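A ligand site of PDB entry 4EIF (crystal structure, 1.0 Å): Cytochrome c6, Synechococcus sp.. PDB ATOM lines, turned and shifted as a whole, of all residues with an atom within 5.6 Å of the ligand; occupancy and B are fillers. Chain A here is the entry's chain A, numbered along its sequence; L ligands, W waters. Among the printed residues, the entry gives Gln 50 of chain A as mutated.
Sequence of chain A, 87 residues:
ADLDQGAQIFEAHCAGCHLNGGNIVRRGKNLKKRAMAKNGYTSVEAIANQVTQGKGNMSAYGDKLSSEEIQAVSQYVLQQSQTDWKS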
ATOM      1  N   ILE A   9      27.693 -26.773  -0.076  1.00  0.00           N
ATOM      2  CA  ILE A   9      27.324 -25.391   0.215  1.00  0.00           C
ATOM      3  C   ILE A   9      26.485 -25.336   1.488  1.00  0.00           C
ATOM      4  O   ILE A   9      26.702 -24.488   2.360  1.00  0.00           O
ATOM      5  CB  ILE A   9      26.592 -24.749  -0.968  1.00  0.00           C
ATOM      6  CG1 ILE A   9      27.531 -24.680  -2.194  1.00  0.00           C
ATOM      7  CG2 ILE A   9      26.030 -23.388  -0.619  1.00  0.00           C
ATOM      8  CD1 ILE A   9      26.761 -24.590  -3.519  1.00  0.00           C
ATOM      9  N   PHE A  10      25.518 -26.256   1.612  1.00  0.00           N
ATOM     10  CA  PHE A  10      24.641 -26.297   2.778  1.00  0.00           C
ATOM     11  C   PHE A  10      25.491 -26.507   4.073  1.00  0.00           C
ATOM     12  O   PHE A  10      25.300 -25.818   5.077  1.00  0.00           O
ATOM     13  CB  PHE A  10      23.618 -27.422   2.634  1.00  0.00           C
ATOM     14  CG  PHE A  10      22.549 -27.384   3.684  1.00  0.00           C
ATOM     15  CD1 PHE A  10      22.709 -28.066   4.908  1.00  0.00           C
ATOM     16  CD2 PHE A  10      21.403 -26.596   3.516  1.00  0.00           C
ATOM     17  CE1 PHE A  10      21.771 -27.960   5.906  1.00  0.00           C
ATOM     18  CE2 PHE A  10      20.455 -26.525   4.549  1.00  0.00           C
ATOM     19  CZ  PHE A  10      20.647 -27.220   5.719  1.00  0.00           C
ATOM     20  N   HIS A  13      27.434 -23.194   4.858  1.00  0.00           N
ATOM     21  CA  HIS A  13      26.753 -21.888   4.993  1.00  0.00           C
ATOM     22  C   HIS A  13      25.404 -21.952   5.704  1.00  0.00           C
ATOM     23  O   HIS A  13      24.906 -20.865   6.041  1.00  0.00           O
ATOM     24  CB  HIS A  13      26.555 -21.254   3.588  1.00  0.00           C
ATOM     25  CG  HIS A  13      27.846 -20.927   2.939  1.00  0.00           C
ATOM     26  ND1 HIS A  13      28.594 -19.819   3.264  1.00  0.00           N
ATOM     27  CD2 HIS A  13      28.572 -21.630   2.052  1.00  0.00           C
ATOM     28  CE1 HIS A  13      29.718 -19.839   2.582  1.00  0.00           C
ATOM     29  NE2 HIS A  13      29.740 -20.929   1.831  1.00  0.00           N
ATOM     30  N   CYS A  14      24.805 -23.127   5.859  1.00  0.00           N
ATOM     31  CA  CYS A  14      23.428 -23.198   6.310  1.00  0.00           C
ATOM     32  C   CYS A  14      23.274 -24.066   7.561  1.00  0.00           C
ATOM     33  O   CYS A  14      22.350 -23.878   8.356  1.00  0.00           O
ATOM     34  CB  CYS A  14      22.507 -23.778   5.208  1.00  0.00           C
ATOM     35  SG  CYS A  14      22.745 -23.077   3.563  1.00  0.00           S
ATOM     36  N   ALA A  15      24.164 -25.050   7.717  1.00  0.00           N
ATOM     37  CA  ALA A  15      24.036 -26.047   8.799  1.00  0.00           C
ATOM     38  C   ALA A  15      24.212 -25.489  10.167  1.00  0.00           C
ATOM     39  O   ALA A  15      23.794 -26.130  11.155  1.00  0.00           O
ATOM     40  CB  ALA A  15      25.026 -27.196   8.512  1.00  0.00           C
ATOM     41  N   GLY A  16      24.784 -24.300  10.328  1.00  0.00           N
ATOM     42  CA  GLY A  16      24.873 -23.692  11.640  1.00  0.00           C
ATOM     43  C   GLY A  16      23.510 -23.526  12.276  1.00  0.00           C
ATOM     44  O   GLY A  16      23.346 -23.665  13.501  1.00  0.00           O
ATOM     45  N   CYS A  17      22.484 -23.212  11.477  1.00  0.00           N
ATOM     46  CA  CYS A  17      21.129 -23.008  11.977  1.00  0.00           C
ATOM     47  C   CYS A  17      20.154 -24.115  11.564  1.00  0.00           C
ATOM     48  O   CYS A  17      19.112 -24.259  12.241  1.00  0.00           O
ATOM     49  CB  CYS A  17      20.562 -21.673  11.504  1.00  0.00           C
ATOM     50  SG  CYS A  17      21.632 -20.327  12.100  1.00  0.00           S
ATOM     51  N   HIS A  18      20.451 -24.824  10.472  1.00  0.00           N
ATOM     52  CA  HIS A  18      19.524 -25.736   9.866  1.00  0.00           C
ATOM     53  C   HIS A  18      20.063 -27.188   9.773  1.00  0.00           C
ATOM     54  O   HIS A  18      19.665 -27.949   8.888  1.00  0.00           O
ATOM     55  CB  HIS A  18      19.088 -25.289   8.462  1.00  0.00           C
ATOM     56  CG  HIS A  18      18.380 -23.959   8.390  1.00  0.00           C
ATOM     57  ND1 HIS A  18      17.131 -23.734   8.932  1.00  0.00           N
ATOM     58  CD2 HIS A  18      18.710 -22.835   7.722  1.00  0.00           C
ATOM     59  CE1 HIS A  18      16.728 -22.504   8.523  1.00  0.00           C
ATOM     60  NE2 HIS A  18      17.676 -21.939   7.793  1.00  0.00           N
ATOM     61  N   ASN A  23      15.626 -25.852  12.520  1.00  0.00           N
ATOM     62  CA  ASN A  23      15.834 -24.390  12.647  1.00  0.00           C
ATOM     63  C   ASN A  23      15.973 -24.098  14.142  1.00  0.00           C
ATOM     64  O   ASN A  23      14.985 -24.056  14.868  1.00  0.00           O
ATOM     65  CB  ASN A  23      14.705 -23.562  12.033  1.00  0.00           C
ATOM     66  CG  ASN A  23      15.066 -22.076  11.988  1.00  0.00           C
ATOM     67  OD1 ASN A  23      15.853 -21.596  12.795  1.00  0.00           O
ATOM     68  ND2 ASN A  23      14.487 -21.351  11.010  1.00  0.00           N
ATOM     69  N   VAL A  25      16.873 -21.441  15.551  1.00  0.00           N
ATOM     70  CA  VAL A  25      16.572 -20.039  15.869  1.00  0.00           C
ATOM     71  C   VAL A  25      15.070 -19.735  15.914  1.00  0.00           C
ATOM     72  O   VAL A  25      14.609 -19.269  16.991  1.00  0.00           O
ATOM     73  CB  VAL A  25      17.180 -19.127  14.793  1.00  0.00           C
ATOM     74  CG1 VAL A  25      16.933 -17.640  15.113  1.00  0.00           C
ATOM     75  CG2 VAL A  25      18.688 -19.383  14.634  1.00  0.00           C
ATOM     76  N   ARG A  26      14.350 -20.037  14.825  1.00  0.00           N
ATOM     77  CA  ARG A  26      12.910 -19.838  14.707  1.00  0.00           C
ATOM     78  C   ARG A  26      12.267 -21.192  14.594  1.00  0.00           C
ATOM     79  O   ARG A  26      12.247 -21.831  13.535  1.00  0.00           O
ATOM     80  CB  ARG A  26      12.518 -18.941  13.523  1.00  0.00           C
ATOM     81  CG  ARG A  26      11.037 -18.616  13.486  1.00  0.00           C
ATOM     82  CD  ARG A  26      10.689 -17.438  12.618  1.00  0.00           C
ATOM     83  NE  ARG A  26       9.256 -17.168  12.725  1.00  0.00           N
ATOM     84  CZ  ARG A  26       8.608 -16.125  12.222  1.00  0.00           C
ATOM     85  NH1 ARG A  26       9.256 -15.182  11.536  1.00  0.00           N
ATOM     86  NH2 ARG A  26       7.294 -16.034  12.393  1.00  0.00           N
ATOM     87  N   GLY A  28       9.295 -22.413  14.289  1.00  0.00           N
ATOM     88  CA  GLY A  28       8.266 -22.730  13.308  1.00  0.00           C
ATOM     89  C   GLY A  28       8.667 -22.609  11.850  1.00  0.00           C
ATOM     90  O   GLY A  28       7.782 -22.703  10.965  1.00  0.00           O
ATOM     91  N   LYS A  29       9.944 -22.387  11.577  1.00  0.00           N
ATOM     92  CA  LYS A  29      10.422 -22.220  10.174  1.00  0.00           C
ATOM     93  C   LYS A  29      11.593 -23.137   9.796  1.00  0.00           C
ATOM     94  O   LYS A  29      12.633 -22.673   9.320  1.00  0.00           O
ATOM     95  CB  LYS A  29      10.712 -20.719   9.848  1.00  0.00           C
ATOM     96  CG  LYS A  29       9.381 -19.922   9.751  1.00  0.00           C
ATOM     97  CD  LYS A  29       9.449 -18.619   9.027  1.00  0.00           C
ATOM     98  CE  LYS A  29       8.147 -17.931   9.032  1.00  0.00           C
ATOM     99  NZ  LYS A  29       8.226 -16.720   8.179  1.00  0.00           N
ATOM    100  N   ASN A  30      11.412 -24.440   9.989  1.00  0.00           N
ATOM    101  CA  ASN A  30      12.396 -25.428   9.491  1.00  0.00           C
ATOM    102  C   ASN A  30      12.313 -25.857   8.029  1.00  0.00           C
ATOM    103  O   ASN A  30      11.488 -25.335   7.251  1.00  0.00           O
ATOM    104  CB  ASN A  30      12.557 -26.566  10.513  1.00  0.00           C
ATOM    105  CG  ASN A  30      11.456 -27.626  10.435  1.00  0.00           C
ATOM    106  OD1 ASN A  30      10.800 -27.771   9.406  1.00  0.00           O
ATOM    107  ND2 ASN A  30      11.348 -28.405  11.493  1.00  0.00           N
ATOM    108  N   LEU A  31      13.226 -26.744   7.644  1.00  0.00           N
ATOM    109  CA  LEU A  31      13.373 -27.146   6.259  1.00  0.00           C
ATOM    110  C   LEU A  31      12.755 -28.514   5.996  1.00  0.00           C
ATOM    111  O   LEU A  31      12.985 -29.116   4.942  1.00  0.00           O
ATOM    112  CB  LEU A  31      14.817 -27.136   5.799  1.00  0.00           C
ATOM    113  CG  LEU A  31      15.629 -25.868   6.166  1.00  0.00           C
ATOM    114  CD1 LEU A  31      17.031 -25.948   5.565  1.00  0.00           C
ATOM    115  CD2 LEU A  31      14.947 -24.594   5.787  1.00  0.00           C
ATOM    116  N   ALA A  35       6.548 -27.547   7.402  1.00  0.00           N
ATOM    117  CA  ALA A  35       6.745 -26.107   7.400  1.00  0.00           C
ATOM    118  C   ALA A  35       7.039 -25.582   6.017  1.00  0.00           C
ATOM    119  O   ALA A  35       6.543 -24.518   5.610  1.00  0.00           O
ATOM    120  CB  ALA A  35       7.854 -25.692   8.388  1.00  0.00           C
ATOM    121  N   MET A  36       7.851 -26.324   5.261  1.00  0.00           N
ATOM    122  CA  MET A  36       8.172 -25.896   3.900  1.00  0.00           C
ATOM    123  C   MET A  36       6.919 -25.825   3.011  1.00  0.00           C
ATOM    124  O   MET A  36       6.711 -24.865   2.262  1.00  0.00           O
ATOM    125  CB  MET A  36       9.241 -26.804   3.285  1.00  0.00           C
ATOM    126  CG  MET A  36      10.593 -26.663   4.005  1.00  0.00           C
ATOM    127  SD  MET A  36      11.522 -25.149   3.582  1.00  0.00           S
ATOM    128  CE  MET A  36      12.221 -25.697   1.995  1.00  0.00           C
ATOM    129  N   ASN A  39       4.529 -22.878   4.007  1.00  0.00           N
ATOM    130  CA  ASN A  39       5.049 -21.591   3.570  1.00  0.00           C
ATOM    131  C   ASN A  39       5.339 -21.489   2.084  1.00  0.00           C
ATOM    132  O   ASN A  39       5.745 -20.450   1.590  1.00  0.00           O
ATOM    133  CB  ASN A  39       6.262 -21.209   4.427  1.00  0.00           C
ATOM    134  CG  ASN A  39       5.867 -20.992   5.886  1.00  0.00           C
ATOM    135  OD1 ASN A  39       6.445 -21.587   6.775  1.00  0.00           O
ATOM    136  ND2 ASN A  39       4.984 -20.136   6.134  1.00  0.00           N
ATOM    137  N   TYR A  41       7.553 -23.177   0.142  1.00  0.00           N
ATOM    138  CA  TYR A  41       8.909 -23.436  -0.323  1.00  0.00           C
ATOM    139  C   TYR A  41       8.975 -24.819  -0.951  1.00  0.00           C
ATOM    140  O   TYR A  41       9.573 -25.768  -0.432  1.00  0.00           O
ATOM    141  CB  TYR A  41       9.911 -23.273   0.833  1.00  0.00           C
ATOM    142  CG  TYR A  41       9.975 -21.848   1.307  1.00  0.00           C
ATOM    143  CD1 TYR A  41      10.540 -20.854   0.535  1.00  0.00           C
ATOM    144  CD2 TYR A  41       9.436 -21.483   2.531  1.00  0.00           C
ATOM    145  CE1 TYR A  41      10.570 -19.528   0.972  1.00  0.00           C
ATOM    146  CE2 TYR A  41       9.435 -20.168   2.974  1.00  0.00           C
ATOM    147  CZ  TYR A  41       9.968 -19.186   2.155  1.00  0.00           C
ATOM    148  OH  TYR A  41       9.992 -17.849   2.542  1.00  0.00           O
ATOM    149  N   ILE A  47      12.665 -21.082  -2.952  1.00  0.00           N
ATOM    150  CA  ILE A  47      13.754 -21.210  -2.010  1.00  0.00           C
ATOM    151  C   ILE A  47      14.910 -20.237  -2.346  1.00  0.00           C
ATOM    152  O   ILE A  47      15.414 -19.516  -1.476  1.00  0.00           O
ATOM    153  CB  ILE A  47      14.238 -22.693  -1.902  1.00  0.00           C
ATOM    154  CG1 ILE A  47      13.124 -23.570  -1.335  1.00  0.00           C
ATOM    155  CG2 ILE A  47      15.522 -22.799  -1.048  1.00  0.00           C
ATOM    156  CD1 ILE A  47      13.318 -25.059  -1.619  1.00  0.00           C
ATOM    157  N   GLN A  50      14.258 -16.590  -1.353  1.00  0.00           N
ATOM    158  CA  GLN A  50      14.378 -16.369   0.075  1.00  0.00           C
ATOM    159  C   GLN A  50      15.859 -16.361   0.493  1.00  0.00           C
ATOM    160  O   GLN A  50      16.267 -15.479   1.280  1.00  0.00           O
ATOM    161  CB  GLN A  50      13.517 -17.349   0.799  1.00  0.00           C
ATOM    162  CG  GLN A  50      13.333 -17.056   2.241  1.00  0.00           C
ATOM    163  CD  GLN A  50      14.380 -17.692   3.099  1.00  0.00           C
ATOM    164  OE1 GLN A  50      15.403 -18.213   2.639  1.00  0.00           O
ATOM    165  NE2 GLN A  50      14.163 -17.590   4.446  1.00  0.00           N
ATOM    166  N   VAL A  51      16.656 -17.265  -0.044  1.00  0.00           N
ATOM    167  CA  VAL A  51      18.067 -17.340   0.321  1.00  0.00           C
ATOM    168  C   VAL A  51      18.788 -16.073  -0.154  1.00  0.00           C
ATOM    169  O   VAL A  51      19.669 -15.539   0.529  1.00  0.00           O
ATOM    170  CB  VAL A  51      18.692 -18.620  -0.290  1.00  0.00           C
ATOM    171  CG1 VAL A  51      20.213 -18.593  -0.236  1.00  0.00           C
ATOM    172  CG2 VAL A  51      18.121 -19.891   0.400  1.00  0.00           C
ATOM    173  N   LYS A  55      15.476 -13.042   5.231  1.00  0.00           N
ATOM    174  CA  LYS A  55      14.190 -12.775   5.804  1.00  0.00           C
ATOM    175  C   LYS A  55      14.309 -12.797   7.312  1.00  0.00           C
ATOM    176  O   LYS A  55      14.878 -13.705   7.873  1.00  0.00           O
ATOM    177  CB  LYS A  55      13.185 -13.858   5.351  1.00  0.00           C
ATOM    178  CG  LYS A  55      11.791 -13.489   5.703  1.00  0.00           C
ATOM    179  CD  LYS A  55      10.767 -14.156   4.897  1.00  0.00           C
ATOM    180  CE  LYS A  55       9.402 -13.453   5.175  1.00  0.00           C
ATOM    181  NZ  LYS A  55       8.345 -14.225   4.669  1.00  0.00           N
ATOM    182  N   GLY A  56      13.707 -11.833   7.990  1.00  0.00           N
ATOM    183  CA  GLY A  56      13.789 -11.734   9.429  1.00  0.00           C
ATOM    184  C   GLY A  56      15.241 -11.775   9.916  1.00  0.00           C
ATOM    185  O   GLY A  56      16.086 -11.045   9.421  1.00  0.00           O
ATOM    186  N   ASN A  57      15.532 -12.669  10.826  1.00  0.00           N
ATOM    187  CA  ASN A  57      16.857 -12.873  11.379  1.00  0.00           C
ATOM    188  C   ASN A  57      17.765 -13.733  10.513  1.00  0.00           C
ATOM    189  O   ASN A  57      18.935 -13.924  10.900  1.00  0.00           O
ATOM    190  CB  ASN A  57      16.736 -13.453  12.819  1.00  0.00           C
ATOM    191  CG  ASN A  57      16.204 -12.444  13.780  1.00  0.00           C
ATOM    192  OD1 ASN A  57      16.607 -11.285  13.750  1.00  0.00           O
ATOM    193  ND2 ASN A  57      15.244 -12.868  14.568  1.00  0.00           N
ATOM    194  N   MET A  58      17.288 -14.255   9.412  1.00  0.00           N
ATOM    195  CA  MET A  58      18.159 -14.938   8.442  1.00  0.00           C
ATOM    196  C   MET A  58      18.806 -13.912   7.501  1.00  0.00           C
ATOM    197  O   MET A  58      18.105 -13.080   6.901  1.00  0.00           O
ATOM    198  CB  MET A  58      17.401 -15.975   7.640  1.00  0.00           C
ATOM    199  CG  MET A  58      18.298 -16.755   6.692  1.00  0.00           C
ATOM    200  SD  MET A  58      17.377 -18.071   5.836  1.00  0.00           S
ATOM    201  CE  MET A  58      18.223 -18.081   4.227  1.00  0.00           C
ATOM    202  N   TYR A  61      21.928 -13.864   1.358  1.00  0.00           N
ATOM    203  CA  TYR A  61      23.093 -14.540   0.751  1.00  0.00           C
ATOM    204  C   TYR A  61      23.416 -14.040  -0.647  1.00  0.00           C
ATOM    205  O   TYR A  61      24.427 -14.467  -1.215  1.00  0.00           O
ATOM    206  CB  TYR A  61      22.984 -16.079   0.797  1.00  0.00           C
ATOM    207  CG  TYR A  61      23.073 -16.594   2.230  1.00  0.00           C
ATOM    208  CD1 TYR A  61      24.291 -17.022   2.730  1.00  0.00           C
ATOM    209  CD2 TYR A  61      21.969 -16.592   3.061  1.00  0.00           C
ATOM    210  CE1 TYR A  61      24.408 -17.416   4.086  1.00  0.00           C
ATOM    211  CE2 TYR A  61      22.053 -16.979   4.380  1.00  0.00           C
ATOM    212  CZ  TYR A  61      23.285 -17.354   4.897  1.00  0.00           C
ATOM    213  OH  TYR A  61      23.355 -17.682   6.238  1.00  0.00           O
ATOM    214  N   LEU A  65      27.060 -15.691  -1.788  1.00  0.00           N
ATOM    215  CA  LEU A  65      27.076 -16.871  -2.637  1.00  0.00           C
ATOM    216  C   LEU A  65      26.692 -16.451  -4.048  1.00  0.00           C
ATOM    217  O   LEU A  65      25.856 -15.575  -4.223  1.00  0.00           O
ATOM    218  CB  LEU A  65      26.097 -17.925  -2.138  1.00  0.00           C
ATOM    219  CG  LEU A  65      26.382 -18.528  -0.777  1.00  0.00           C
ATOM    220  CD1 LEU A  65      25.206 -19.424  -0.351  1.00  0.00           C
ATOM    221  CD2 LEU A  65      27.663 -19.359  -0.813  1.00  0.00           C
ATOM    222  N   VAL A  73      22.278 -25.002  -3.828  1.00  0.00           N
ATOM    223  CA  VAL A  73      21.834 -25.268  -2.446  1.00  0.00           C
ATOM    224  C   VAL A  73      20.306 -25.296  -2.357  1.00  0.00           C
ATOM    225  O   VAL A  73      19.747 -26.044  -1.557  1.00  0.00           O
ATOM    226  CB  VAL A  73      22.468 -24.299  -1.413  1.00  0.00           C
ATOM    227  CG1 VAL A  73      21.885 -22.888  -1.450  1.00  0.00           C
ATOM    228  CG2 VAL A  73      22.389 -24.893  -0.017  1.00  0.00           C
ATOM    229  N   VAL A  77      18.068 -28.336  -0.811  1.00  0.00           N
ATOM    230  CA  VAL A  77      17.062 -28.149   0.208  1.00  0.00           C
ATOM    231  C   VAL A  77      15.682 -28.636  -0.273  1.00  0.00           C
ATOM    232  O   VAL A  77      14.932 -29.267   0.502  1.00  0.00           O
ATOM    233  CB  VAL A  77      17.020 -26.658   0.661  1.00  0.00           C
ATOM    234  CG1 VAL A  77      15.796 -26.366   1.495  1.00  0.00           C
ATOM    235  CG2 VAL A  77      18.313 -26.320   1.433  1.00  0.00           C
HETATM  236 FE1  LIG L   1      17.598 -20.134   6.905  1.00  0.00          FE
HETATM  237  C1  LIG L   1      14.228 -19.701   7.268  1.00  0.00           C
HETATM  238  C2  LIG L   1      17.091 -21.728   3.930  1.00  0.00           C
HETATM  239  C3  LIG L   1      20.946 -20.225   6.410  1.00  0.00           C
HETATM  240  C4  LIG L   1      18.093 -18.831  10.022  1.00  0.00           C
HETATM  241  N1  LIG L   1      15.985 -20.659   5.845  1.00  0.00           N
HETATM  242  C5  LIG L   1      14.653 -20.424   6.170  1.00  0.00           C
HETATM  243  C6  LIG L   1      13.794 -20.986   5.156  1.00  0.00           C
HETATM  244  C7  LIG L   1      14.592 -21.520   4.175  1.00  0.00           C
HETATM  245  C8  LIG L   1      15.960 -21.312   4.634  1.00  0.00           C
HETATM  246  C9  LIG L   1      14.187 -22.173   2.875  1.00  0.00           C
HETATM  247  C10 LIG L   1      12.269 -21.003   5.206  1.00  0.00           C
HETATM  248  C11 LIG L   1      11.791 -22.197   6.059  1.00  0.00           C
HETATM  249  C12 LIG L   1      10.303 -22.238   6.326  1.00  0.00           C
HETATM  250  O1  LIG L   1       9.538 -21.321   5.991  1.00  0.00           O
HETATM  251  O2  LIG L   1       9.805 -23.305   6.877  1.00  0.00           O
HETATM  252  N2  LIG L   1      18.786 -20.811   5.443  1.00  0.00           N
HETATM  253  C13 LIG L   1      18.419 -21.482   4.313  1.00  0.00           C
HETATM  254  C14 LIG L   1      19.570 -21.823   3.493  1.00  0.00           C
HETATM  255  C15 LIG L   1      20.635 -21.334   4.153  1.00  0.00           C
HETATM  256  C16 LIG L   1      20.160 -20.737   5.381  1.00  0.00           C
HETATM  257  C17 LIG L   1      19.516 -22.625   2.204  1.00  0.00           C
HETATM  258  C18 LIG L   1      22.125 -21.344   3.737  1.00  0.00           C
HETATM  259  C19 LIG L   1      22.425 -20.643   2.472  1.00  0.00           C
HETATM  260  N3  LIG L   1      19.209 -19.629   7.985  1.00  0.00           N
HETATM  261  C20 LIG L   1      20.504 -19.817   7.644  1.00  0.00           C
HETATM  262  C21 LIG L   1      21.374 -19.563   8.765  1.00  0.00           C
HETATM  263  C22 LIG L   1      20.579 -19.158   9.805  1.00  0.00           C
HETATM  264  C23 LIG L   1      19.222 -19.203   9.293  1.00  0.00           C
HETATM  265  C24 LIG L   1      22.856 -19.816   8.764  1.00  0.00           C
HETATM  266  C25 LIG L   1      20.968 -18.821  11.242  1.00  0.00           C
HETATM  267  C26 LIG L   1      21.938 -17.739  11.429  1.00  0.00           C
HETATM  268  N4  LIG L   1      16.413 -19.389   8.347  1.00  0.00           N
HETATM  269  C27 LIG L   1      16.799 -18.813   9.542  1.00  0.00           C
HETATM  270  C28 LIG L   1      15.673 -18.212  10.217  1.00  0.00           C
HETATM  271  C29 LIG L   1      14.565 -18.423   9.377  1.00  0.00           C
HETATM  272  C30 LIG L   1      15.033 -19.174   8.262  1.00  0.00           C
HETATM  273  C31 LIG L   1      15.760 -17.449  11.488  1.00  0.00           C
HETATM  274  C32 LIG L   1      13.188 -17.813   9.562  1.00  0.00           C
HETATM  275  C33 LIG L   1      13.126 -16.422   8.874  1.00  0.00           C
HETATM  276  C34 LIG L   1      11.771 -15.842   9.050  1.00  0.00           C
HETATM  277  O3  LIG L   1      11.495 -15.142  10.060  1.00  0.00           O
HETATM  278  O4  LIG L   1      10.918 -16.024   8.165  1.00  0.00           O
HETATM  279  O   HOH W   1      11.520 -17.575   6.027  1.00  0.00           O
HETATM  280  O   HOH W   2      13.253 -14.188  11.825  1.00  0.00           O
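C18 of the ligand is bonded to SG of Cys 14 (1.8 Å). The side-chain sulfur (SG) of Cys 17 is bonded to a carbon (C25) of the ligand. An iron atom (FE1) of the ligand is bound by a ring nitrogen (NE2) of His 18 (2.0 Å). The side-chain sulfur (SD) of Met 58 is bound to an iron atom (FE1) of the ligand (2.3 Å). An oxygen (O2) of the ligand sits close to the backbone carbonyl oxygen of Asn 30 (2.7 Å). The guanidinium group of Arg 26 is in salt-bridge range of an oxygen (O3) of the ligand (2.7 Å). NZ of Lys 29 lies within salt-bridge range of O4 of the ligand (2.8 Å). The side-chain amide oxygen (OD1) of Asn 39 lies close to an oxygen (O1) of the ligand, at 3.2 Å.
SD of Met 58 sits close to NE2 of Gln 50 (3.5 Å). The backbone NH (N) of Arg 26 lies within hydrogen-bond range of the side-chain amide oxygen (OD1) of Asn 23, at 3.0 Å. ND2 of Asn 23 lies within hydrogen-bond range of O of Lys 29 (2.8 Å). The side-chain amide oxygen (OD1) of Asn 39 lies close to the backbone carbonyl oxygen (O) of Ala 35, at 3.2 Å. The backbone carbonyl oxygen (O) of Met 36 is in hydrogen-bond range of the backbone NH (N) of Tyr 41. The backbone NH (N) of Tyr 61 is in hydrogen-bond range of the backbone carbonyl oxygen (O) of Val 51. The backbone NH (N) of Val 25 lies within hydrogen-bond range of the side-chain amide oxygen (OD1) of Asn 23, 2.9 Å away.
Residues that only touch the ligand: His 13 (3.6 Å), Asn 23 (3.4 Å), Val 25 (3.8 Å), Leu 31 (3.5 Å), Ala 35 (3.4 Å), Met 36 (3.9 Å), Tyr 41 (3.2 Å), Gln 50 (3.4 Å), Val 51 (3.6 Å), Lys 55 (3.4 Å), Tyr 61 (3.3 Å) and Val 77 (3.96 Å). 20 residues have an atom within 4 Å of the ligand: His 13, Cys 14, Cys 17, His 18, Asn 23, Val 25, Arg 26, Lys 29, Asn 30, Leu 31, Ala 35, Met 36, Asn 39, Tyr 41, Gln 50, Val 51, Lys 55, Met 58, Tyr 61 and Val 77.
Water W2 bridges O3 of the ligand (2.7 Å) and N of Asn 57 (2.9 Å). Water W1 lies within hydrogen-bond range of an oxygen (O4) of the ligand (2.7 Å) and the side-chain amide nitrogen of Gln 50 (3.1 Å).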
